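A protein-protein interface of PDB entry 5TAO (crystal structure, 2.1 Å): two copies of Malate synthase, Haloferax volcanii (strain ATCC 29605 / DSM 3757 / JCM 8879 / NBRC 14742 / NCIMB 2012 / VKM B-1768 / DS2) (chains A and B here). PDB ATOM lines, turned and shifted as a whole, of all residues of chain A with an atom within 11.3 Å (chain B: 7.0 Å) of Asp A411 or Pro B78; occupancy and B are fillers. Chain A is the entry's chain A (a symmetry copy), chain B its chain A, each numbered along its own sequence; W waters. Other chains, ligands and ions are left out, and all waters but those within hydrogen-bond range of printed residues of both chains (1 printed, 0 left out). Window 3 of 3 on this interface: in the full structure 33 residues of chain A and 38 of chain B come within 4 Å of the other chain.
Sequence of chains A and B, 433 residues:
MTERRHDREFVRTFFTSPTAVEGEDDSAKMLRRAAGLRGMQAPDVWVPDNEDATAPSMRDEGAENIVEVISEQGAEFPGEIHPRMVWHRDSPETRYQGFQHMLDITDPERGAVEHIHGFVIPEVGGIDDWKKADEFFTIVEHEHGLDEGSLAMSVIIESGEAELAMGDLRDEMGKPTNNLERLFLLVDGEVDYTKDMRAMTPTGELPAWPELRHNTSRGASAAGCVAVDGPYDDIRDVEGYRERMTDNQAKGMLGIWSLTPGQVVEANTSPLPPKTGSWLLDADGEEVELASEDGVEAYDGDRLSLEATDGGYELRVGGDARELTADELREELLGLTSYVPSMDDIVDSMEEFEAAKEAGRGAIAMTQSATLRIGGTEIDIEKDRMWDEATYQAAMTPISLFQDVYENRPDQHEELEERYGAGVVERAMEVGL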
ATOM      1  N   PHE A 402     -26.267 -13.892 -20.359  1.00  0.00           N
ATOM      2  CA  PHE A 402     -25.006 -14.148 -19.601  1.00  0.00           C
ATOM      3  C   PHE A 402     -24.814 -13.083 -18.501  1.00  0.00           C
ATOM      4  O   PHE A 402     -24.495 -13.403 -17.383  1.00  0.00           O
ATOM      5  CB  PHE A 402     -23.771 -14.185 -20.503  1.00  0.00           C
ATOM      6  CG  PHE A 402     -22.514 -14.302 -19.723  1.00  0.00           C
ATOM      7  CD1 PHE A 402     -22.117 -15.530 -19.219  1.00  0.00           C
ATOM      8  CD2 PHE A 402     -21.806 -13.172 -19.371  1.00  0.00           C
ATOM      9  CE1 PHE A 402     -20.985 -15.633 -18.454  1.00  0.00           C
ATOM     10  CE2 PHE A 402     -20.684 -13.265 -18.581  1.00  0.00           C
ATOM     11  CZ  PHE A 402     -20.280 -14.481 -18.123  1.00  0.00           C
ATOM     12  N   ASP A 404     -27.097 -11.161 -16.993  1.00  0.00           N
ATOM     13  CA  ASP A 404     -28.117 -11.230 -15.940  1.00  0.00           C
ATOM     14  C   ASP A 404     -27.676 -12.283 -14.984  1.00  0.00           C
ATOM     15  O   ASP A 404     -27.823 -12.165 -13.763  1.00  0.00           O
ATOM     16  CB  ASP A 404     -29.477 -11.604 -16.562  1.00  0.00           C
ATOM     17  CG  ASP A 404     -30.626 -11.491 -15.588  1.00  0.00           C
ATOM     18  OD1 ASP A 404     -30.787 -10.413 -15.017  1.00  0.00           O
ATOM     19  OD2 ASP A 404     -31.355 -12.486 -15.392  1.00  0.00           O
ATOM     20  N   VAL A 405     -27.122 -13.356 -15.527  1.00  0.00           N
ATOM     21  CA  VAL A 405     -26.655 -14.430 -14.692  1.00  0.00           C
ATOM     22  C   VAL A 405     -25.492 -13.924 -13.824  1.00  0.00           C
ATOM     23  O   VAL A 405     -25.504 -14.101 -12.588  1.00  0.00           O
ATOM     24  CB  VAL A 405     -26.249 -15.650 -15.528  1.00  0.00           C
ATOM     25  CG1 VAL A 405     -25.429 -16.609 -14.721  1.00  0.00           C
ATOM     26  CG2 VAL A 405     -27.476 -16.383 -16.089  1.00  0.00           C
ATOM     27  N   TYR A 406     -24.530 -13.273 -14.459  1.00  0.00           N
ATOM     28  CA  TYR A 406     -23.324 -12.793 -13.749  1.00  0.00           C
ATOM     29  C   TYR A 406     -23.699 -11.780 -12.651  1.00  0.00           C
ATOM     30  O   TYR A 406     -23.301 -11.949 -11.519  1.00  0.00           O
ATOM     31  CB  TYR A 406     -22.278 -12.206 -14.708  1.00  0.00           C
ATOM     32  CG  TYR A 406     -20.868 -11.964 -14.085  1.00  0.00           C
ATOM     33  CD1 TYR A 406     -19.876 -12.957 -14.109  1.00  0.00           C
ATOM     34  CD2 TYR A 406     -20.541 -10.746 -13.508  1.00  0.00           C
ATOM     35  CE1 TYR A 406     -18.634 -12.742 -13.551  1.00  0.00           C
ATOM     36  CE2 TYR A 406     -19.293 -10.522 -12.969  1.00  0.00           C
ATOM     37  CZ  TYR A 406     -18.357 -11.523 -12.993  1.00  0.00           C
ATOM     38  OH  TYR A 406     -17.124 -11.287 -12.460  1.00  0.00           O
ATOM     39  N   GLU A 407     -24.521 -10.790 -12.958  1.00  0.00           N
ATOM     40  CA  GLU A 407     -24.976  -9.879 -11.924  1.00  0.00           C
ATOM     41  C   GLU A 407     -25.693 -10.547 -10.772  1.00  0.00           C
ATOM     42  O   GLU A 407     -25.611 -10.059  -9.669  1.00  0.00           O
ATOM     43  CB  GLU A 407     -25.902  -8.811 -12.500  1.00  0.00           C
ATOM     44  CG  GLU A 407     -25.184  -7.605 -13.093  1.00  0.00           C
ATOM     45  CD  GLU A 407     -25.923  -6.968 -14.269  1.00  0.00           C
ATOM     46  OE1 GLU A 407     -26.853  -7.578 -14.821  1.00  0.00           O
ATOM     47  OE2 GLU A 407     -25.560  -5.853 -14.659  1.00  0.00           O
ATOM     48  N   ASN A 408     -26.418 -11.645 -10.998  1.00  0.00           N
ATOM     49  CA  ASN A 408     -27.274 -12.190  -9.933  1.00  0.00           C
ATOM     50  C   ASN A 408     -26.831 -13.468  -9.317  1.00  0.00           C
ATOM     51  O   ASN A 408     -27.383 -13.914  -8.297  1.00  0.00           O
ATOM     52  CB  ASN A 408     -28.683 -12.384 -10.480  1.00  0.00           C
ATOM     53  CG  ASN A 408     -29.368 -11.067 -10.735  1.00  0.00           C
ATOM     54  OD1 ASN A 408     -29.853 -10.435  -9.792  1.00  0.00           O
ATOM     55  ND2 ASN A 408     -29.401 -10.636 -11.986  1.00  0.00           N
ATOM     56  N   ARG A 409     -25.855 -14.098  -9.927  1.00  0.00           N
ATOM     57  CA  ARG A 409     -25.330 -15.309  -9.359  1.00  0.00           C
ATOM     58  C   ARG A 409     -23.788 -15.224  -9.055  1.00  0.00           C
ATOM     59  O   ARG A 409     -22.983 -15.869  -9.725  1.00  0.00           O
ATOM     60  CB  ARG A 409     -25.654 -16.450 -10.313  1.00  0.00           C
ATOM     61  CG  ARG A 409     -27.139 -16.581 -10.627  1.00  0.00           C
ATOM     62  CD  ARG A 409     -27.886 -16.950  -9.392  1.00  0.00           C
ATOM     63  NE  ARG A 409     -27.290 -18.155  -8.852  1.00  0.00           N
ATOM     64  CZ  ARG A 409     -27.594 -19.379  -9.240  1.00  0.00           C
ATOM     65  NH1 ARG A 409     -28.459 -19.595 -10.210  1.00  0.00           N
ATOM     66  NH2 ARG A 409     -27.013 -20.413  -8.680  1.00  0.00           N
ATOM     67  N   PRO A 410     -23.402 -14.436  -8.022  1.00  0.00           N
ATOM     68  CA  PRO A 410     -22.001 -14.426  -7.527  1.00  0.00           C
ATOM     69  C   PRO A 410     -21.502 -15.840  -7.218  1.00  0.00           C
ATOM     70  O   PRO A 410     -20.390 -16.178  -7.581  1.00  0.00           O
ATOM     71  CB  PRO A 410     -22.070 -13.551  -6.270  1.00  0.00           C
ATOM     72  CG  PRO A 410     -23.500 -13.573  -5.847  1.00  0.00           C
ATOM     73  CD  PRO A 410     -24.275 -13.631  -7.145  1.00  0.00           C
ATOM     74  N   ASP A 411     -22.366 -16.698  -6.695  1.00  0.00           N
ATOM     75  CA  ASP A 411     -22.018 -18.098  -6.530  1.00  0.00           C
ATOM     76  C   ASP A 411     -21.622 -18.849  -7.770  1.00  0.00           C
ATOM     77  O   ASP A 411     -21.249 -20.028  -7.664  1.00  0.00           O
ATOM     78  CB  ASP A 411     -23.142 -18.875  -5.840  1.00  0.00           C
ATOM     79  CG  ASP A 411     -24.358 -19.097  -6.771  1.00  0.00           C
ATOM     80  OD1 ASP A 411     -24.772 -18.106  -7.338  1.00  0.00           O
ATOM     81  OD2 ASP A 411     -24.793 -20.241  -6.963  1.00  0.00           O
ATOM     82  N   GLN A 412     -21.721 -18.234  -8.943  1.00  0.00           N
ATOM     83  CA  GLN A 412     -21.397 -18.938 -10.186  1.00  0.00           C
ATOM     84  C   GLN A 412     -20.204 -18.376 -10.898  1.00  0.00           C
ATOM     85  O   GLN A 412     -19.850 -18.915 -11.923  1.00  0.00           O
ATOM     86  CB  GLN A 412     -22.591 -18.963 -11.183  1.00  0.00           C
ATOM     87  CG  GLN A 412     -23.560 -20.071 -10.834  1.00  0.00           C
ATOM     88  CD  GLN A 412     -24.820 -20.201 -11.750  1.00  0.00           C
ATOM     89  OE1 GLN A 412     -24.955 -19.589 -12.816  1.00  0.00           O
ATOM     90  NE2 GLN A 412     -25.671 -21.061 -11.346  1.00  0.00           N
ATOM     91  N   HIS A 413     -19.590 -17.322 -10.364  1.00  0.00           N
ATOM     92  CA  HIS A 413     -18.476 -16.644 -11.022  1.00  0.00           C
ATOM     93  C   HIS A 413     -17.261 -17.532 -11.270  1.00  0.00           C
ATOM     94  O   HIS A 413     -16.593 -17.382 -12.281  1.00  0.00           O
ATOM     95  CB  HIS A 413     -18.063 -15.409 -10.219  1.00  0.00           C
ATOM     96  CG  HIS A 413     -19.107 -14.341 -10.219  1.00  0.00           C
ATOM     97  ND1 HIS A 413     -18.847 -13.036  -9.882  1.00  0.00           N
ATOM     98  CD2 HIS A 413     -20.419 -14.386 -10.544  1.00  0.00           C
ATOM     99  CE1 HIS A 413     -19.947 -12.321  -9.987  1.00  0.00           C
ATOM    100  NE2 HIS A 413     -20.917 -13.119 -10.388  1.00  0.00           N
ATOM    101  N   GLU A 414     -17.026 -18.476 -10.375  1.00  0.00           N
ATOM    102  CA  GLU A 414     -15.871 -19.354 -10.482  1.00  0.00           C
ATOM    103  C   GLU A 414     -16.049 -20.367 -11.612  1.00  0.00           C
ATOM    104  O   GLU A 414     -15.158 -20.549 -12.428  1.00  0.00           O
ATOM    105  CB  GLU A 414     -15.634 -20.080  -9.153  1.00  0.00           C
ATOM    106  CG  GLU A 414     -14.390 -20.956  -9.124  1.00  0.00           C
ATOM    107  CD  GLU A 414     -14.632 -22.298  -8.457  1.00  0.00           C
ATOM    108  OE1 GLU A 414     -14.122 -22.470  -7.327  1.00  0.00           O
ATOM    109  OE2 GLU A 414     -15.330 -23.173  -9.052  1.00  0.00           O
ATOM    110  N   GLU A 415     -17.192 -21.048 -11.649  1.00  0.00           N
ATOM    111  CA  GLU A 415     -17.471 -21.965 -12.754  1.00  0.00           C
ATOM    112  C   GLU A 415     -17.537 -21.183 -14.076  1.00  0.00           C
ATOM    113  O   GLU A 415     -17.197 -21.706 -15.133  1.00  0.00           O
ATOM    114  CB  GLU A 415     -18.747 -22.734 -12.481  1.00  0.00           C
ATOM    115  CG  GLU A 415     -18.533 -23.896 -11.519  1.00  0.00           C
ATOM    116  CD  GLU A 415     -19.759 -24.312 -10.721  1.00  0.00           C
ATOM    117  OE1 GLU A 415     -20.237 -25.485 -10.847  1.00  0.00           O
ATOM    118  OE2 GLU A 415     -20.195 -23.472  -9.910  1.00  0.00           O
ATOM    119  N   LEU A 416     -17.962 -19.926 -14.038  1.00  0.00           N
ATOM    120  CA  LEU A 416     -18.048 -19.181 -15.298  1.00  0.00           C
ATOM    121  C   LEU A 416     -16.687 -18.791 -15.829  1.00  0.00           C
ATOM    122  O   LEU A 416     -16.416 -18.919 -17.044  1.00  0.00           O
ATOM    123  CB  LEU A 416     -18.939 -17.941 -15.181  1.00  0.00           C
ATOM    124  CG  LEU A 416     -20.467 -18.192 -15.070  1.00  0.00           C
ATOM    125  CD1 LEU A 416     -21.224 -16.881 -15.215  1.00  0.00           C
ATOM    126  CD2 LEU A 416     -21.005 -19.223 -16.070  1.00  0.00           C
ATOM    127  N   GLU A 417     -15.835 -18.287 -14.940  1.00  0.00           N
ATOM    128  CA  GLU A 417     -14.456 -17.938 -15.343  1.00  0.00           C
ATOM    129  C   GLU A 417     -13.707 -19.171 -15.827  1.00  0.00           C
ATOM    130  O   GLU A 417     -13.094 -19.172 -16.884  1.00  0.00           O
ATOM    131  CB  GLU A 417     -13.728 -17.230 -14.217  1.00  0.00           C
ATOM    132  CG  GLU A 417     -13.982 -15.723 -14.269  1.00  0.00           C
ATOM    133  CD  GLU A 417     -13.878 -15.083 -12.910  1.00  0.00           C
ATOM    134  OE1 GLU A 417     -14.848 -14.386 -12.515  1.00  0.00           O
ATOM    135  OE2 GLU A 417     -12.843 -15.314 -12.239  1.00  0.00           O
ATOM    136  N   GLU A 418     -13.860 -20.256 -15.102  1.00  0.00           N
ATOM    137  CA  GLU A 418     -13.296 -21.486 -15.528  1.00  0.00           C
ATOM    138  C   GLU A 418     -13.868 -21.933 -16.870  1.00  0.00           C
ATOM    139  O   GLU A 418     -13.168 -22.555 -17.687  1.00  0.00           O
ATOM    140  CB  GLU A 418     -13.518 -22.515 -14.420  1.00  0.00           C
ATOM    141  CG  GLU A 418     -12.679 -23.771 -14.529  1.00  0.00           C
ATOM    142  CD  GLU A 418     -13.551 -25.000 -14.744  1.00  0.00           C
ATOM    143  OE1 GLU A 418     -13.334 -25.717 -15.745  1.00  0.00           O
ATOM    144  OE2 GLU A 418     -14.472 -25.232 -13.919  1.00  0.00           O
ATOM    145  N   ARG B   8     -35.162 -10.633 -11.865  1.00  0.00           N
ATOM    146  CA  ARG B   8     -34.509 -11.546 -12.800  1.00  0.00           C
ATOM    147  C   ARG B   8     -35.162 -11.362 -14.123  1.00  0.00           C
ATOM    148  O   ARG B   8     -36.323 -11.629 -14.283  1.00  0.00           O
ATOM    149  CB  ARG B   8     -34.601 -13.001 -12.356  1.00  0.00           C
ATOM    150  CG  ARG B   8     -33.618 -13.467 -11.250  1.00  0.00           C
ATOM    151  CD  ARG B   8     -32.142 -13.066 -11.410  1.00  0.00           C
ATOM    152  NE  ARG B   8     -31.520 -13.574 -12.635  1.00  0.00           N
ATOM    153  CZ  ARG B   8     -30.987 -14.770 -12.826  1.00  0.00           C
ATOM    154  NH1 ARG B   8     -30.940 -15.685 -11.859  1.00  0.00           N
ATOM    155  NH2 ARG B   8     -30.458 -15.023 -14.005  1.00  0.00           N
ATOM    156  N   ALA B  34     -31.536 -29.119  -0.747  1.00  0.00           N
ATOM    157  CA  ALA B  34     -31.738 -28.262  -1.943  1.00  0.00           C
ATOM    158  C   ALA B  34     -31.313 -26.921  -1.580  1.00  0.00           C
ATOM    159  O   ALA B  34     -30.657 -26.216  -2.322  1.00  0.00           O
ATOM    160  CB  ALA B  34     -33.214 -28.272  -2.325  1.00  0.00           C
ATOM    161  N   ALA B  35     -31.613 -26.543  -0.350  1.00  0.00           N
ATOM    162  CA  ALA B  35     -31.188 -25.214   0.120  1.00  0.00           C
ATOM    163  C   ALA B  35     -29.699 -24.985   0.216  1.00  0.00           C
ATOM    164  O   ALA B  35     -29.227 -23.825   0.169  1.00  0.00           O
ATOM    165  CB  ALA B  35     -31.838 -24.925   1.455  1.00  0.00           C
ATOM    166  N   GLY B  36     -28.931 -26.076   0.333  1.00  0.00           N
ATOM    167  CA  GLY B  36     -27.457 -25.956   0.293  1.00  0.00           C
ATOM    168  C   GLY B  36     -26.789 -25.903  -1.061  1.00  0.00           C
ATOM    169  O   GLY B  36     -25.584 -25.655  -1.148  1.00  0.00           O
ATOM    170  N   LEU B  37     -27.550 -26.094  -2.140  1.00  0.00           N
ATOM    171  CA  LEU B  37     -26.961 -26.144  -3.470  1.00  0.00           C
ATOM    172  C   LEU B  37     -26.366 -24.828  -3.782  1.00  0.00           C
ATOM    173  O   LEU B  37     -26.897 -23.798  -3.361  1.00  0.00           O
ATOM    174  CB  LEU B  37     -28.036 -26.535  -4.542  1.00  0.00           C
ATOM    175  CG  LEU B  37     -28.637 -27.918  -4.382  1.00  0.00           C
ATOM    176  CD1 LEU B  37     -29.835 -28.188  -5.326  1.00  0.00           C
ATOM    177  CD2 LEU B  37     -27.555 -28.981  -4.512  1.00  0.00           C
ATOM    178  N   ARG B  38     -25.254 -24.830  -4.512  1.00  0.00           N
ATOM    179  CA  ARG B  38     -24.558 -23.601  -4.881  1.00  0.00           C
ATOM    180  C   ARG B  38     -23.968 -23.742  -6.262  1.00  0.00           C
ATOM    181  O   ARG B  38     -23.868 -24.831  -6.809  1.00  0.00           O
ATOM    182  CB  ARG B  38     -23.426 -23.278  -3.873  1.00  0.00           C
ATOM    183  CG  ARG B  38     -23.866 -23.117  -2.403  1.00  0.00           C
ATOM    184  CD  ARG B  38     -24.344 -21.677  -2.099  1.00  0.00           C
ATOM    185  NE  ARG B  38     -24.814 -21.572  -0.725  1.00  0.00           N
ATOM    186  CZ  ARG B  38     -25.911 -22.119  -0.240  1.00  0.00           C
ATOM    187  NH1 ARG B  38     -26.768 -22.756  -1.014  1.00  0.00           N
ATOM    188  NH2 ARG B  38     -26.196 -21.981   1.049  1.00  0.00           N
ATOM    189  N   GLY B  39     -23.547 -22.643  -6.834  1.00  0.00           N
ATOM    190  CA  GLY B  39     -23.003 -22.681  -8.165  1.00  0.00           C
ATOM    191  C   GLY B  39     -23.950 -23.269  -9.205  1.00  0.00           C
ATOM    192  O   GLY B  39     -25.203 -23.234  -9.070  1.00  0.00           O
ATOM    193  N   MET B  40     -23.348 -23.845 -10.229  1.00  0.00           N
ATOM    194  CA  MET B  40     -24.089 -24.293 -11.365  1.00  0.00           C
ATOM    195  C   MET B  40     -25.146 -25.294 -10.979  1.00  0.00           C
ATOM    196  O   MET B  40     -26.096 -25.522 -11.752  1.00  0.00           O
ATOM    197  CB  MET B  40     -23.152 -24.891 -12.428  1.00  0.00           C
ATOM    198  CG  MET B  40     -22.400 -23.838 -13.212  1.00  0.00           C
ATOM    199  SD  MET B  40     -23.425 -22.697 -14.192  1.00  0.00           S
ATOM    200  CE  MET B  40     -23.838 -23.837 -15.498  1.00  0.00           C
ATOM    201  N   GLN B  41     -25.010 -25.923  -9.814  1.00  0.00           N
ATOM    202  CA  GLN B  41     -26.005 -26.914  -9.346  1.00  0.00           C
ATOM    203  C   GLN B  41     -27.212 -26.247  -8.676  1.00  0.00           C
ATOM    204  O   GLN B  41     -28.158 -26.914  -8.300  1.00  0.00           O
ATOM    205  CB  GLN B  41     -25.420 -27.829  -8.261  1.00  0.00           C
ATOM    206  CG  GLN B  41     -24.346 -28.822  -8.667  1.00  0.00           C
ATOM    207  CD  GLN B  41     -24.113 -29.826  -7.547  1.00  0.00           C
ATOM    208  OE1 GLN B  41     -24.029 -29.463  -6.360  1.00  0.00           O
ATOM    209  NE2 GLN B  41     -24.093 -31.098  -7.907  1.00  0.00           N
ATOM    210  N   ALA B  42     -27.120 -24.952  -8.426  1.00  0.00           N
ATOM    211  CA  ALA B  42     -28.214 -24.235  -7.764  1.00  0.00           C
ATOM    212  C   ALA B  42     -29.076 -23.442  -8.777  1.00  0.00           C
ATOM    213  O   ALA B  42     -28.533 -22.774  -9.654  1.00  0.00           O
ATOM    214  CB  ALA B  42     -27.655 -23.312  -6.723  1.00  0.00           C
ATOM    215  N   PRO B  43     -30.433 -23.531  -8.639  1.00  0.00           N
ATOM    216  CA  PRO B  43     -31.397 -22.984  -9.656  1.00  0.00           C
ATOM    217  C   PRO B  43     -31.547 -21.482  -9.587  1.00  0.00           C
ATOM    218  O   PRO B  43     -31.398 -20.887  -8.521  1.00  0.00           O
ATOM    219  CB  PRO B  43     -32.706 -23.708  -9.304  1.00  0.00           C
ATOM    220  CG  PRO B  43     -32.614 -23.955  -7.831  1.00  0.00           C
ATOM    221  CD  PRO B  43     -31.135 -24.348  -7.650  1.00  0.00           C
ATOM    222  N   ASP B  44     -31.843 -20.834 -10.708  1.00  0.00           N
ATOM    223  CA  ASP B  44     -32.197 -19.466 -10.662  1.00  0.00           C
ATOM    224  C   ASP B  44     -33.438 -19.306  -9.796  1.00  0.00           C
ATOM    225  O   ASP B  44     -33.545 -18.377  -9.005  1.00  0.00           O
ATOM    226  CB  ASP B  44     -32.387 -18.941 -12.058  1.00  0.00           C
ATOM    227  CG  ASP B  44     -31.074 -18.705 -12.762  1.00  0.00           C
ATOM    228  OD1 ASP B  44     -30.036 -18.431 -12.086  1.00  0.00           O
ATOM    229  OD2 ASP B  44     -31.092 -18.682 -13.991  1.00  0.00           O
ATOM    230  N   GLY B  74     -32.593 -19.883   4.387  1.00  0.00           N
ATOM    231  CA  GLY B  74     -33.026 -19.060   3.301  1.00  0.00           C
ATOM    232  C   GLY B  74     -32.137 -17.927   2.967  1.00  0.00           C
ATOM    233  O   GLY B  74     -31.864 -17.733   1.821  1.00  0.00           O
ATOM    234  N   ALA B  75     -31.562 -17.232   3.948  1.00  0.00           N
ATOM    235  CA  ALA B  75     -30.633 -16.078   3.658  1.00  0.00           C
ATOM    236  C   ALA B  75     -29.475 -16.344   2.760  1.00  0.00           C
ATOM    237  O   ALA B  75     -28.967 -15.439   2.075  1.00  0.00           O
ATOM    238  CB  ALA B  75     -30.092 -15.456   4.967  1.00  0.00           C
ATOM    239  N   GLU B  76     -29.002 -17.574   2.765  1.00  0.00           N
ATOM    240  CA  GLU B  76     -27.740 -17.881   2.072  1.00  0.00           C
ATOM    241  C   GLU B  76     -28.004 -18.401   0.641  1.00  0.00           C
ATOM    242  O   GLU B  76     -27.080 -18.497  -0.200  1.00  0.00           O
ATOM    243  CB  GLU B  76     -27.019 -18.983   2.890  1.00  0.00           C
ATOM    244  CG  GLU B  76     -26.724 -18.590   4.358  1.00  0.00           C
ATOM    245  CD  GLU B  76     -25.830 -17.374   4.388  1.00  0.00           C
ATOM    246  OE1 GLU B  76     -25.286 -17.063   3.295  1.00  0.00           O
ATOM    247  OE2 GLU B  76     -25.705 -16.711   5.431  1.00  0.00           O
ATOM    248  N   PHE B  77     -29.266 -18.754   0.381  1.00  0.00           N
ATOM    249  CA  PHE B  77     -29.634 -19.330  -0.916  1.00  0.00           C
ATOM    250  C   PHE B  77     -29.323 -18.300  -2.007  1.00  0.00           C
ATOM    251  O   PHE B  77     -29.729 -17.171  -1.907  1.00  0.00           O
ATOM    252  CB  PHE B  77     -31.079 -19.825  -0.922  1.00  0.00           C
ATOM    253  CG  PHE B  77     -31.384 -20.698  -2.076  1.00  0.00           C
ATOM    254  CD1 PHE B  77     -30.931 -21.983  -2.098  1.00  0.00           C
ATOM    255  CD2 PHE B  77     -32.033 -20.196  -3.203  1.00  0.00           C
ATOM    256  CE1 PHE B  77     -31.170 -22.805  -3.191  1.00  0.00           C
ATOM    257  CE2 PHE B  77     -32.237 -21.003  -4.316  1.00  0.00           C
ATOM    258  CZ  PHE B  77     -31.833 -22.319  -4.304  1.00  0.00           C
ATOM    259  N   PRO B  78     -28.543 -18.695  -3.033  1.00  0.00           N
ATOM    260  CA  PRO B  78     -28.054 -17.829  -4.065  1.00  0.00           C
ATOM    261  C   PRO B  78     -29.101 -17.417  -5.165  1.00  0.00           C
ATOM    262  O   PRO B  78     -28.943 -16.380  -5.828  1.00  0.00           O
ATOM    263  CB  PRO B  78     -26.957 -18.661  -4.682  1.00  0.00           C
ATOM    264  CG  PRO B  78     -27.386 -20.040  -4.527  1.00  0.00           C
ATOM    265  CD  PRO B  78     -28.165 -20.101  -3.286  1.00  0.00           C
ATOM    266  N   GLY B  79     -30.086 -18.243  -5.363  1.00  0.00           N
ATOM    267  CA  GLY B  79     -31.204 -17.941  -6.281  1.00  0.00           C
ATOM    268  C   GLY B  79     -32.406 -17.370  -5.543  1.00  0.00           C
ATOM    269  O   GLY B  79     -32.284 -16.906  -4.428  1.00  0.00           O
ATOM    270  N   GLU B  80     -33.580 -17.385  -6.183  1.00  0.00           N
ATOM    271  CA  GLU B  80     -34.752 -16.771  -5.608  1.00  0.00           C
ATOM    272  C   GLU B  80     -35.590 -17.907  -5.237  1.00  0.00           C
ATOM    273  O   GLU B  80     -35.594 -18.922  -5.909  1.00  0.00           O
ATOM    274  CB  GLU B  80     -35.523 -15.956  -6.640  1.00  0.00           C
ATOM    275  CG  GLU B  80     -34.919 -14.611  -7.057  1.00  0.00           C
ATOM    276  CD  GLU B  80     -35.920 -13.795  -7.937  1.00  0.00           C
ATOM    277  OE1 GLU B  80     -37.123 -14.185  -8.093  1.00  0.00           O
ATOM    278  OE2 GLU B  80     -35.519 -12.750  -8.479  1.00  0.00           O
ATOM    279  N   ILE B  81     -36.333 -17.737  -4.171  1.00  0.00           N
ATOM    280  CA  ILE B  81     -37.178 -18.770  -3.662  1.00  0.00           C
ATOM    281  C   ILE B  81     -38.727 -18.479  -3.867  1.00  0.00           C
ATOM    282  O   ILE B  81     -39.284 -17.520  -3.373  1.00  0.00           O
ATOM    283  CB  ILE B  81     -36.877 -18.965  -2.189  1.00  0.00           C
ATOM    284  CG1 ILE B  81     -35.328 -19.097  -1.946  1.00  0.00           C
ATOM    285  CG2 ILE B  81     -37.589 -20.176  -1.669  1.00  0.00           C
ATOM    286  CD1 ILE B  81     -34.971 -19.324  -0.507  1.00  0.00           C
HETATM  287  O   HOH W   1     -21.794 -26.705  -9.071  1.00  0.00           O
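O of Ala B35 is in hydrogen-bond range of NH1 of Arg B38, 2.9 Å away. The side-chain amide nitrogen (ND2) of Asn A408 lies within hydrogen-bond range of the backbone carbonyl oxygen (O) of Asp A404, 2.8 Å away. The side-chain carboxylate (OD2) of Asp A411 is in salt-bridge range of the guanidinium group (NH2) of Arg A409, at 2.8 Å. NH2 of Arg A409 lies close to NE2 of Gln A412, at 3.1 Å.
Of the 20 printed residues of chain B, 8 touch a printed residue of chain A. Printed residues of chain B that touch a printed residue of chain A: Arg B8, Arg B38, Gly B39, Met B40, Ala B42, Pro B43, Asp B44 and Pro B78. Hydrophobic or aromatic side chains of chain B within 4 Å of the printed part of chain A: Met B40, Ala B42 and Pro B78. Along chain B the printed residues that touch a printed residue of chain A span positions 8 to 78. Hydrophobic or aromatic side chains of chain A that line the printed part of chain B: Val A405. Among the printed residues, 17 pairs touch across the chains. Among the printed residues, Asp or Glu carboxylates within 4 Å of a Lys or Arg side-chain nitrogen of the other chain: Asp A404 with Arg B8 (3.0 Å) and Arg A409 with Asp B44 (2.7 Å).
No position is printed for both chains. Of the 17 pairs that touch across the chains among the printed residues, none has its exchanged pair printed and touching as well.
Asp A411 touches three residues of chain B. Pro B78 touches just these residues of chain A: Asn A408 (3.8 Å), Arg A409 (3.8 Å) and Asp A411 (3.4 Å). Arg B38 touches just one residue of chain A: Asp A411. Of chain A, only Arg A409 (3.4 Å), Asp A411 (2.7 Å), Gln A412 (3.2 Å) and Glu A415 (3.4 Å) come within 4 Å of Gly B39. Ala B42 touches two residues of chain A. No residue of chain A comes within 4 Å of Phe B77. No residue of chain A comes within 4 Å of Gly B79. Of the printed residues of chain B, Val A405 touches Arg B8. Of the printed residues of chain B, Glu A415 touches Gly B39 and Met B40. Of the printed residues of chain B, Arg A409 touches Gly B39 (3.4 Å), Ala B42 (3.0 Å), Pro B43 (3.6 Å), Asp B44 (2.7 Å) and Pro B78 (3.8 Å). Printed residues of chain B within 4 Å of Asp A404: Arg B8 (3.0 Å). Of the printed residues of chain A, Asp B44 touches Arg A409. Pro A410 touches none of the printed residues of chain B. The nearest printed residue of chain A that does not touch Pro B43 is Gln A412 (6.0 Å).
The guanidinium group (NE) of Arg B8 lies within salt-bridge range of the side-chain carboxylate (OD2) of Asp A404 (3.0 Å). O of Gly B39 is in hydrogen-bond range of NH2 of Arg A409, 3.4 Å away. The backbone NH (N) of Gly B39 sits at hydrogen-bond distance from the side-chain carboxylate (OD2) of Asp A411, at 2.7 Å. The backbone carbonyl oxygen (O) of Gly B39 lies within hydrogen-bond range of the side-chain amide nitrogen (NE2) of Gln A412, 3.2 Å away. The side-chain sulfur (SD) of Met B40 sits close to the side-chain amide oxygen (OE1) of Gln A412 (3.7 Å). OE2 of Glu A415 sits at hydrogen-bond distance from N of Met B40, at 3.2 Å. O of Ala B42 is in hydrogen-bond range of NH2 of Arg A409, 3.0 Å away. The side-chain carboxylate (OD1) of Asp B44 lies within salt-bridge range of the guanidinium group (NH1) of Arg A409, 2.7 Å away.
Water W1 lies within hydrogen-bond range of OE1 of Glu A415 (2.7 Å), N of Gln B41 (3.4 Å) and N of Met B40 (3.5 Å).
Among the printed residues, pairs that only touch across the chains: Asp A411 with Pro B78 (3.4 Å), Glu A415 with Gly B39 (3.4 Å), Asn A408 with Arg B8 (3.5 Å), Arg A409 with Pro B43 (3.6 Å), Asp A411 with Arg B38 (3.7 Å), Gln A412 with Ala B42 (3.7 Å), Arg A409 with Pro B78 (3.8 Å), Asn A408 with Pro B78 (3.8 Å) and Val A405 with Arg B8 (3.9 Å).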
